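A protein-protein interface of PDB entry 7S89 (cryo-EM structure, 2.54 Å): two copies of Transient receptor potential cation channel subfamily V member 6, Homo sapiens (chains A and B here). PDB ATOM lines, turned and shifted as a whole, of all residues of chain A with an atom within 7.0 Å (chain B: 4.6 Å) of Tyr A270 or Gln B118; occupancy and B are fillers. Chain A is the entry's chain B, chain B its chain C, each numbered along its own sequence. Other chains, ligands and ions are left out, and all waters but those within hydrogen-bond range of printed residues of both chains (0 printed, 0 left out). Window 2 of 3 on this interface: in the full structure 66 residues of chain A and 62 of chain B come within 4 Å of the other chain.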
ATOM      1  N   TRP A 268     -27.688   3.886  13.392  1.00  0.00           N
ATOM      2  CA  TRP A 268     -26.496   4.487  13.983  1.00  0.00           C
ATOM      3  C   TRP A 268     -26.887   5.169  15.287  1.00  0.00           C
ATOM      4  O   TRP A 268     -28.068   5.324  15.606  1.00  0.00           O
ATOM      5  CB  TRP A 268     -25.777   5.468  13.053  1.00  0.00           C
ATOM      6  CG  TRP A 268     -26.618   6.456  12.277  1.00  0.00           C
ATOM      7  CD1 TRP A 268     -26.935   6.380  10.960  1.00  0.00           C
ATOM      8  CD2 TRP A 268     -27.252   7.640  12.769  1.00  0.00           C
ATOM      9  NE1 TRP A 268     -27.705   7.441  10.592  1.00  0.00           N
ATOM     10  CE2 TRP A 268     -27.915   8.237  11.685  1.00  0.00           C
ATOM     11  CE3 TRP A 268     -27.321   8.257  14.024  1.00  0.00           C
ATOM     12  CZ2 TRP A 268     -28.652   9.407  11.819  1.00  0.00           C
ATOM     13  CZ3 TRP A 268     -28.046   9.428  14.147  1.00  0.00           C
ATOM     14  CH2 TRP A 268     -28.703   9.985  13.049  1.00  0.00           C
ATOM     15  N   THR A 269     -25.870   5.556  16.050  1.00  0.00           N
ATOM     16  CA  THR A 269     -26.011   6.351  17.262  1.00  0.00           C
ATOM     17  C   THR A 269     -25.030   7.511  17.197  1.00  0.00           C
ATOM     18  O   THR A 269     -23.823   7.296  17.051  1.00  0.00           O
ATOM     19  CB  THR A 269     -25.752   5.498  18.508  1.00  0.00           C
ATOM     20  OG1 THR A 269     -26.704   4.434  18.560  1.00  0.00           O
ATOM     21  CG2 THR A 269     -25.859   6.332  19.762  1.00  0.00           C
ATOM     22  N   TYR A 270     -25.547   8.741  17.297  1.00  0.00           N
ATOM     23  CA  TYR A 270     -24.723   9.959  17.223  1.00  0.00           C
ATOM     24  C   TYR A 270     -24.948  10.722  18.519  1.00  0.00           C
ATOM     25  O   TYR A 270     -25.774  11.637  18.578  1.00  0.00           O
ATOM     26  CB  TYR A 270     -25.086  10.755  16.034  1.00  0.00           C
ATOM     27  CG  TYR A 270     -24.191  11.938  15.796  1.00  0.00           C
ATOM     28  CD1 TYR A 270     -22.882  11.766  15.365  1.00  0.00           C
ATOM     29  CD2 TYR A 270     -24.675  13.229  15.936  1.00  0.00           C
ATOM     30  CE1 TYR A 270     -22.071  12.847  15.117  1.00  0.00           C
ATOM     31  CE2 TYR A 270     -23.879  14.312  15.688  1.00  0.00           C
ATOM     32  CZ  TYR A 270     -22.576  14.118  15.279  1.00  0.00           C
ATOM     33  OH  TYR A 270     -21.794  15.218  15.038  1.00  0.00           O
ATOM     34  N   GLY A 271     -24.180  10.349  19.535  1.00  0.00           N
ATOM     35  CA  GLY A 271     -24.359  10.819  20.880  1.00  0.00           C
ATOM     36  C   GLY A 271     -25.742  10.514  21.408  1.00  0.00           C
ATOM     37  O   GLY A 271     -26.140   9.357  21.565  1.00  0.00           O
ATOM     38  N   PRO A 272     -26.508  11.571  21.674  1.00  0.00           N
ATOM     39  CA  PRO A 272     -27.900  11.382  22.105  1.00  0.00           C
ATOM     40  C   PRO A 272     -28.830  10.928  20.993  1.00  0.00           C
ATOM     41  O   PRO A 272     -29.921  10.425  21.280  1.00  0.00           O
ATOM     42  CB  PRO A 272     -28.279  12.771  22.621  1.00  0.00           C
ATOM     43  CG  PRO A 272     -27.415  13.697  21.832  1.00  0.00           C
ATOM     44  CD  PRO A 272     -26.124  12.990  21.625  1.00  0.00           C
ATOM     45  N   LEU A 273     -28.451  11.112  19.734  1.00  0.00           N
ATOM     46  CA  LEU A 273     -29.311  10.691  18.638  1.00  0.00           C
ATOM     47  C   LEU A 273     -29.206   9.196  18.380  1.00  0.00           C
ATOM     48  O   LEU A 273     -28.206   8.555  18.708  1.00  0.00           O
ATOM     49  CB  LEU A 273     -28.967  11.445  17.362  1.00  0.00           C
ATOM     50  CG  LEU A 273     -29.333  12.914  17.321  1.00  0.00           C
ATOM     51  CD1 LEU A 273     -28.791  13.499  16.055  1.00  0.00           C
ATOM     52  CD2 LEU A 273     -30.825  13.048  17.367  1.00  0.00           C
ATOM     53  N   THR A 274     -30.261   8.645  17.786  1.00  0.00           N
ATOM     54  CA  THR A 274     -30.306   7.271  17.321  1.00  0.00           C
ATOM     55  C   THR A 274     -31.225   7.210  16.111  1.00  0.00           C
ATOM     56  O   THR A 274     -32.385   7.607  16.195  1.00  0.00           O
ATOM     57  CB  THR A 274     -30.822   6.314  18.406  1.00  0.00           C
ATOM     58  OG1 THR A 274     -29.998   6.404  19.570  1.00  0.00           O
ATOM     59  CG2 THR A 274     -30.795   4.891  17.922  1.00  0.00           C
ATOM     60  N   SER A 275     -30.715   6.716  14.991  1.00  0.00           N
ATOM     61  CA  SER A 275     -31.548   6.420  13.838  1.00  0.00           C
ATOM     62  C   SER A 275     -31.978   4.968  13.931  1.00  0.00           C
ATOM     63  O   SER A 275     -31.136   4.076  14.056  1.00  0.00           O
ATOM     64  CB  SER A 275     -30.816   6.666  12.528  1.00  0.00           C
ATOM     65  OG  SER A 275     -31.633   6.381  11.417  1.00  0.00           O
ATOM     66  N   GLU A 634     -35.853   8.789  13.951  1.00  0.00           N
ATOM     67  CA  GLU A 634     -34.723   9.372  14.652  1.00  0.00           C
ATOM     68  C   GLU A 634     -35.211   9.943  15.976  1.00  0.00           C
ATOM     69  O   GLU A 634     -36.139  10.753  15.999  1.00  0.00           O
ATOM     70  CB  GLU A 634     -34.052  10.444  13.797  1.00  0.00           C
ATOM     71  CG  GLU A 634     -32.777  10.999  14.384  1.00  0.00           C
ATOM     72  CD  GLU A 634     -32.026  11.899  13.415  1.00  0.00           C
ATOM     73  OE1 GLU A 634     -32.486  12.073  12.268  1.00  0.00           O
ATOM     74  OE2 GLU A 634     -30.972  12.438  13.802  1.00  0.00           O
ATOM     75  N   HIS B  84     -14.264   8.483   9.261  1.00  0.00           N
ATOM     76  CA  HIS B  84     -15.554   8.928   9.771  1.00  0.00           C
ATOM     77  C   HIS B  84     -16.376   7.763  10.311  1.00  0.00           C
ATOM     78  O   HIS B  84     -17.043   7.893  11.343  1.00  0.00           O
ATOM     79  CB  HIS B  84     -16.311   9.653   8.660  1.00  0.00           C
ATOM     80  CG  HIS B  84     -15.773  11.014   8.357  1.00  0.00           C
ATOM     81  ND1 HIS B  84     -16.030  11.669   7.175  1.00  0.00           N
ATOM     82  CD2 HIS B  84     -15.044  11.871   9.109  1.00  0.00           C
ATOM     83  CE1 HIS B  84     -15.457  12.858   7.196  1.00  0.00           C
ATOM     84  NE2 HIS B  84     -14.853  13.006   8.360  1.00  0.00           N
ATOM     85  N   GLU B 108      -9.889  15.457   6.803  1.00  0.00           N
ATOM     86  CA  GLU B 108     -10.880  15.490   5.740  1.00  0.00           C
ATOM     87  C   GLU B 108     -12.263  15.835   6.288  1.00  0.00           C
ATOM     88  O   GLU B 108     -12.667  15.324   7.336  1.00  0.00           O
ATOM     89  CB  GLU B 108     -10.914  14.154   5.010  1.00  0.00           C
ATOM     90  CG  GLU B 108      -9.652  13.879   4.231  1.00  0.00           C
ATOM     91  CD  GLU B 108      -9.469  14.821   3.059  1.00  0.00           C
ATOM     92  OE1 GLU B 108     -10.483  15.237   2.461  1.00  0.00           O
ATOM     93  OE2 GLU B 108      -8.309  15.146   2.736  1.00  0.00           O
ATOM     94  N   PRO B 109     -12.993  16.715   5.623  1.00  0.00           N
ATOM     95  CA  PRO B 109     -14.356  17.023   6.060  1.00  0.00           C
ATOM     96  C   PRO B 109     -15.386  16.128   5.396  1.00  0.00           C
ATOM     97  O   PRO B 109     -15.183  15.668   4.269  1.00  0.00           O
ATOM     98  CB  PRO B 109     -14.531  18.481   5.626  1.00  0.00           C
ATOM     99  CG  PRO B 109     -13.675  18.600   4.430  1.00  0.00           C
ATOM    100  CD  PRO B 109     -12.490  17.706   4.659  1.00  0.00           C
ATOM    101  N   MET B 110     -16.490  15.867   6.088  1.00  0.00           N
ATOM    102  CA  MET B 110     -17.601  15.160   5.468  1.00  0.00           C
ATOM    103  C   MET B 110     -18.289  16.097   4.481  1.00  0.00           C
ATOM    104  O   MET B 110     -18.465  17.286   4.753  1.00  0.00           O
ATOM    105  CB  MET B 110     -18.555  14.669   6.554  1.00  0.00           C
ATOM    106  CG  MET B 110     -19.473  13.553   6.148  1.00  0.00           C
ATOM    107  SD  MET B 110     -20.386  12.928   7.557  1.00  0.00           S
ATOM    108  CE  MET B 110     -19.069  12.230   8.514  1.00  0.00           C
ATOM    109  N   TYR B 115     -24.144  17.037   6.274  1.00  0.00           N
ATOM    110  CA  TYR B 115     -23.048  17.019   7.231  1.00  0.00           C
ATOM    111  C   TYR B 115     -21.816  17.696   6.627  1.00  0.00           C
ATOM    112  O   TYR B 115     -20.727  17.132   6.649  1.00  0.00           O
ATOM    113  CB  TYR B 115     -22.729  15.594   7.648  1.00  0.00           C
ATOM    114  CG  TYR B 115     -23.847  14.843   8.329  1.00  0.00           C
ATOM    115  CD1 TYR B 115     -24.151  15.069   9.656  1.00  0.00           C
ATOM    116  CD2 TYR B 115     -24.570  13.880   7.648  1.00  0.00           C
ATOM    117  CE1 TYR B 115     -25.161  14.384  10.282  1.00  0.00           C
ATOM    118  CE2 TYR B 115     -25.588  13.187   8.264  1.00  0.00           C
ATOM    119  CZ  TYR B 115     -25.876  13.443   9.582  1.00  0.00           C
ATOM    120  OH  TYR B 115     -26.884  12.757  10.211  1.00  0.00           O
ATOM    121  N   GLU B 116     -21.994  18.892   6.076  1.00  0.00           N
ATOM    122  CA  GLU B 116     -20.886  19.594   5.438  1.00  0.00           C
ATOM    123  C   GLU B 116     -19.849  20.040   6.461  1.00  0.00           C
ATOM    124  O   GLU B 116     -20.190  20.564   7.523  1.00  0.00           O
ATOM    125  CB  GLU B 116     -21.400  20.804   4.665  1.00  0.00           C
ATOM    126  CG  GLU B 116     -20.347  21.529   3.850  1.00  0.00           C
ATOM    127  CD  GLU B 116     -20.937  22.663   3.040  1.00  0.00           C
ATOM    128  OE1 GLU B 116     -22.170  22.844   3.098  1.00  0.00           O
ATOM    129  OE2 GLU B 116     -20.176  23.383   2.360  1.00  0.00           O
ATOM    130  N   GLY B 117     -18.580  19.818   6.140  1.00  0.00           N
ATOM    131  CA  GLY B 117     -17.496  20.295   6.977  1.00  0.00           C
ATOM    132  C   GLY B 117     -17.369  19.585   8.301  1.00  0.00           C
ATOM    133  O   GLY B 117     -16.725  20.103   9.215  1.00  0.00           O
ATOM    134  N   GLN B 118     -17.953  18.405   8.431  1.00  0.00           N
ATOM    135  CA  GLN B 118     -17.857  17.641   9.660  1.00  0.00           C
ATOM    136  C   GLN B 118     -16.627  16.755   9.588  1.00  0.00           C
ATOM    137  O   GLN B 118     -16.405  16.072   8.586  1.00  0.00           O
ATOM    138  CB  GLN B 118     -19.102  16.794   9.888  1.00  0.00           C
ATOM    139  CG  GLN B 118     -19.101  16.091  11.218  1.00  0.00           C
ATOM    140  CD  GLN B 118     -20.298  15.203  11.388  1.00  0.00           C
ATOM    141  OE1 GLN B 118     -21.040  14.976  10.442  1.00  0.00           O
ATOM    142  NE2 GLN B 118     -20.524  14.732  12.603  1.00  0.00           N
ATOM    143  N   THR B 119     -15.825  16.780  10.636  1.00  0.00           N
ATOM    144  CA  THR B 119     -14.645  15.946  10.730  1.00  0.00           C
ATOM    145  C   THR B 119     -14.955  14.776  11.643  1.00  0.00           C
ATOM    146  O   THR B 119     -16.019  14.703  12.254  1.00  0.00           O
ATOM    147  CB  THR B 119     -13.451  16.742  11.264  1.00  0.00           C
ATOM    148  OG1 THR B 119     -13.675  17.079  12.638  1.00  0.00           O
ATOM    149  CG2 THR B 119     -13.288  18.019  10.468  1.00  0.00           C
ATOM    150  N   ALA B 120     -14.012  13.843  11.731  1.00  0.00           N
ATOM    151  CA  ALA B 120     -14.166  12.772  12.703  1.00  0.00           C
ATOM    152  C   ALA B 120     -13.874  13.256  14.107  1.00  0.00           C
ATOM    153  O   ALA B 120     -14.223  12.578  15.080  1.00  0.00           O
ATOM    154  CB  ALA B 120     -13.263  11.601  12.351  1.00  0.00           C
ATOM    155  N   HIS B 122     -15.240  16.003  15.230  1.00  0.00           N
ATOM    156  CA  HIS B 122     -16.630  16.268  15.595  1.00  0.00           C
ATOM    157  C   HIS B 122     -17.337  15.014  16.093  1.00  0.00           C
ATOM    158  O   HIS B 122     -18.066  15.059  17.088  1.00  0.00           O
ATOM    159  CB  HIS B 122     -17.394  16.821  14.400  1.00  0.00           C
ATOM    160  CG  HIS B 122     -17.110  18.251  14.085  1.00  0.00           C
ATOM    161  ND1 HIS B 122     -17.715  19.289  14.756  1.00  0.00           N
ATOM    162  CD2 HIS B 122     -16.317  18.820  13.149  1.00  0.00           C
ATOM    163  CE1 HIS B 122     -17.310  20.435  14.246  1.00  0.00           C
ATOM    164  NE2 HIS B 122     -16.458  20.178  13.271  1.00  0.00           N
ATOM    165  N   ILE B 123     -17.143  13.888  15.401  1.00  0.00           N
ATOM    166  CA  ILE B 123     -17.923  12.685  15.681  1.00  0.00           C
ATOM    167  C   ILE B 123     -17.485  12.051  16.992  1.00  0.00           C
ATOM    168  O   ILE B 123     -18.314  11.652  17.816  1.00  0.00           O
ATOM    169  CB  ILE B 123     -17.802  11.693  14.515  1.00  0.00           C
ATOM    170  CG1 ILE B 123     -18.253  12.343  13.217  1.00  0.00           C
ATOM    171  CG2 ILE B 123     -18.650  10.478  14.770  1.00  0.00           C
ATOM    172  CD1 ILE B 123     -17.806  11.602  12.015  1.00  0.00           C
ATOM    173  N   VAL B 126     -18.822  13.928  19.949  1.00  0.00           N
ATOM    174  CA  VAL B 126     -20.240  13.690  20.227  1.00  0.00           C
ATOM    175  C   VAL B 126     -20.439  12.309  20.829  1.00  0.00           C
ATOM    176  O   VAL B 126     -21.181  12.138  21.804  1.00  0.00           O
ATOM    177  CB  VAL B 126     -21.071  13.878  18.947  1.00  0.00           C
ATOM    178  CG1 VAL B 126     -22.504  13.525  19.186  1.00  0.00           C
ATOM    179  CG2 VAL B 126     -21.007  15.293  18.501  1.00  0.00           C
ATOM    180  N   ASN B 127     -19.717  11.318  20.313  1.00  0.00           N
ATOM    181  CA  ASN B 127     -19.713   9.985  20.897  1.00  0.00           C
ATOM    182  C   ASN B 127     -18.944   9.897  22.209  1.00  0.00           C
ATOM    183  O   ASN B 127     -18.973   8.829  22.826  1.00  0.00           O
ATOM    184  CB  ASN B 127     -19.155   8.989  19.888  1.00  0.00           C
ATOM    185  CG  ASN B 127     -20.126   8.699  18.770  1.00  0.00           C
ATOM    186  OD1 ASN B 127     -19.881   9.014  17.611  1.00  0.00           O
ATOM    187  ND2 ASN B 127     -21.253   8.098  19.122  1.00  0.00           N
ATOM    188  N   ALA B 147     -18.863  22.867  11.183  1.00  0.00           N
ATOM    189  CA  ALA B 147     -19.815  21.908  10.631  1.00  0.00           C
ATOM    190  C   ALA B 147     -21.060  22.667  10.190  1.00  0.00           C
ATOM    191  O   ALA B 147     -21.977  22.890  10.981  1.00  0.00           O
ATOM    192  CB  ALA B 147     -20.144  20.835  11.660  1.00  0.00           C
ATOM    193  N   PHE B 152     -26.971  20.185  11.370  1.00  0.00           N
ATOM    194  CA  PHE B 152     -26.464  20.864  12.549  1.00  0.00           C
ATOM    195  C   PHE B 152     -27.113  22.224  12.782  1.00  0.00           C
ATOM    196  O   PHE B 152     -26.928  22.805  13.855  1.00  0.00           O
ATOM    197  CB  PHE B 152     -24.944  21.010  12.441  1.00  0.00           C
ATOM    198  CG  PHE B 152     -24.230  19.700  12.304  1.00  0.00           C
ATOM    199  CD1 PHE B 152     -24.131  18.836  13.382  1.00  0.00           C
ATOM    200  CD2 PHE B 152     -23.655  19.332  11.100  1.00  0.00           C
ATOM    201  CE1 PHE B 152     -23.487  17.627  13.256  1.00  0.00           C
ATOM    202  CE2 PHE B 152     -23.005  18.127  10.971  1.00  0.00           C
ATOM    203  CZ  PHE B 152     -22.919  17.276  12.051  1.00  0.00           C
ATOM    204  N   PHE B 169     -19.558  21.258  20.485  1.00  0.00           N
ATOM    205  CA  PHE B 169     -20.203  19.947  20.525  1.00  0.00           C
ATOM    206  C   PHE B 169     -19.934  19.256  21.854  1.00  0.00           C
ATOM    207  O   PHE B 169     -20.808  18.569  22.393  1.00  0.00           O
ATOM    208  CB  PHE B 169     -19.755  19.026  19.383  1.00  0.00           C
ATOM    209  CG  PHE B 169     -20.262  19.398  18.002  1.00  0.00           C
ATOM    210  CD1 PHE B 169     -20.852  20.612  17.728  1.00  0.00           C
ATOM    211  CD2 PHE B 169     -20.247  18.448  16.998  1.00  0.00           C
ATOM    212  CE1 PHE B 169     -21.326  20.906  16.470  1.00  0.00           C
ATOM    213  CE2 PHE B 169     -20.735  18.732  15.747  1.00  0.00           C
ATOM    214  CZ  PHE B 169     -21.268  19.966  15.485  1.00  0.00           C
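Among the printed residues, merely in contact across the chains: Tyr A270 with Phe B152, Tyr A270 with Val B126, Gly A271 with Val B126, Gly A271 with Asn B127 and Tyr A270 with Phe B169.
The backbone carbonyl oxygen (O) of Thr A269 sits at hydrogen-bond distance from the side-chain amide nitrogen (ND2) of Asn B127 (3.4 Å).
The side-chain hydroxyl (OH) of Tyr A270 is in hydrogen-bond range of the side-chain amide nitrogen (NE2) of Gln B118 (2.8 Å).
Hydrophobic or aromatic side chains of chain B that line the printed part of chain A: Val B126, Phe B152 and Phe B169.
Of the 9 printed residues of chain A, 3 touch a printed residue of chain B.
Hydrophobic or aromatic side chains of chain A within 4 Å of the printed part of chain B: Tyr A270.
Among the printed residues, no Asp or Glu carboxylate lies within 4 Å of a Lys or Arg side-chain nitrogen of the other chain.
Of chain A, only Tyr A270 comes within 4 Å of Gln B118.
Gly B117 touches none of the printed residues of chain A.
Of the printed residues of chain B, Gly A271 touches Val B126 and Asn B127.
Of the printed residues of chain B, Thr A269 touches Asn B127 (3.4 Å).
Of the printed residues of chain A, Asn B127 touches Thr A269 (3.4 Å) and Gly A271 (3.7 Å).
Trp A268 touches none of the printed residues of chain B.
No position is printed for both chains.
The backbone NH (N) of Met B110 sits at hydrogen-bond distance from the backbone carbonyl oxygen (O) of Gln B118.
The backbone carbonyl oxygen of Ile B123 lies close to the side-chain amide oxygen of Asn B127, 3.1 Å away.
The backbone carbonyl oxygen (O) of Gln B118 is in hydrogen-bond range of a ring nitrogen (NE2) of His B84.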
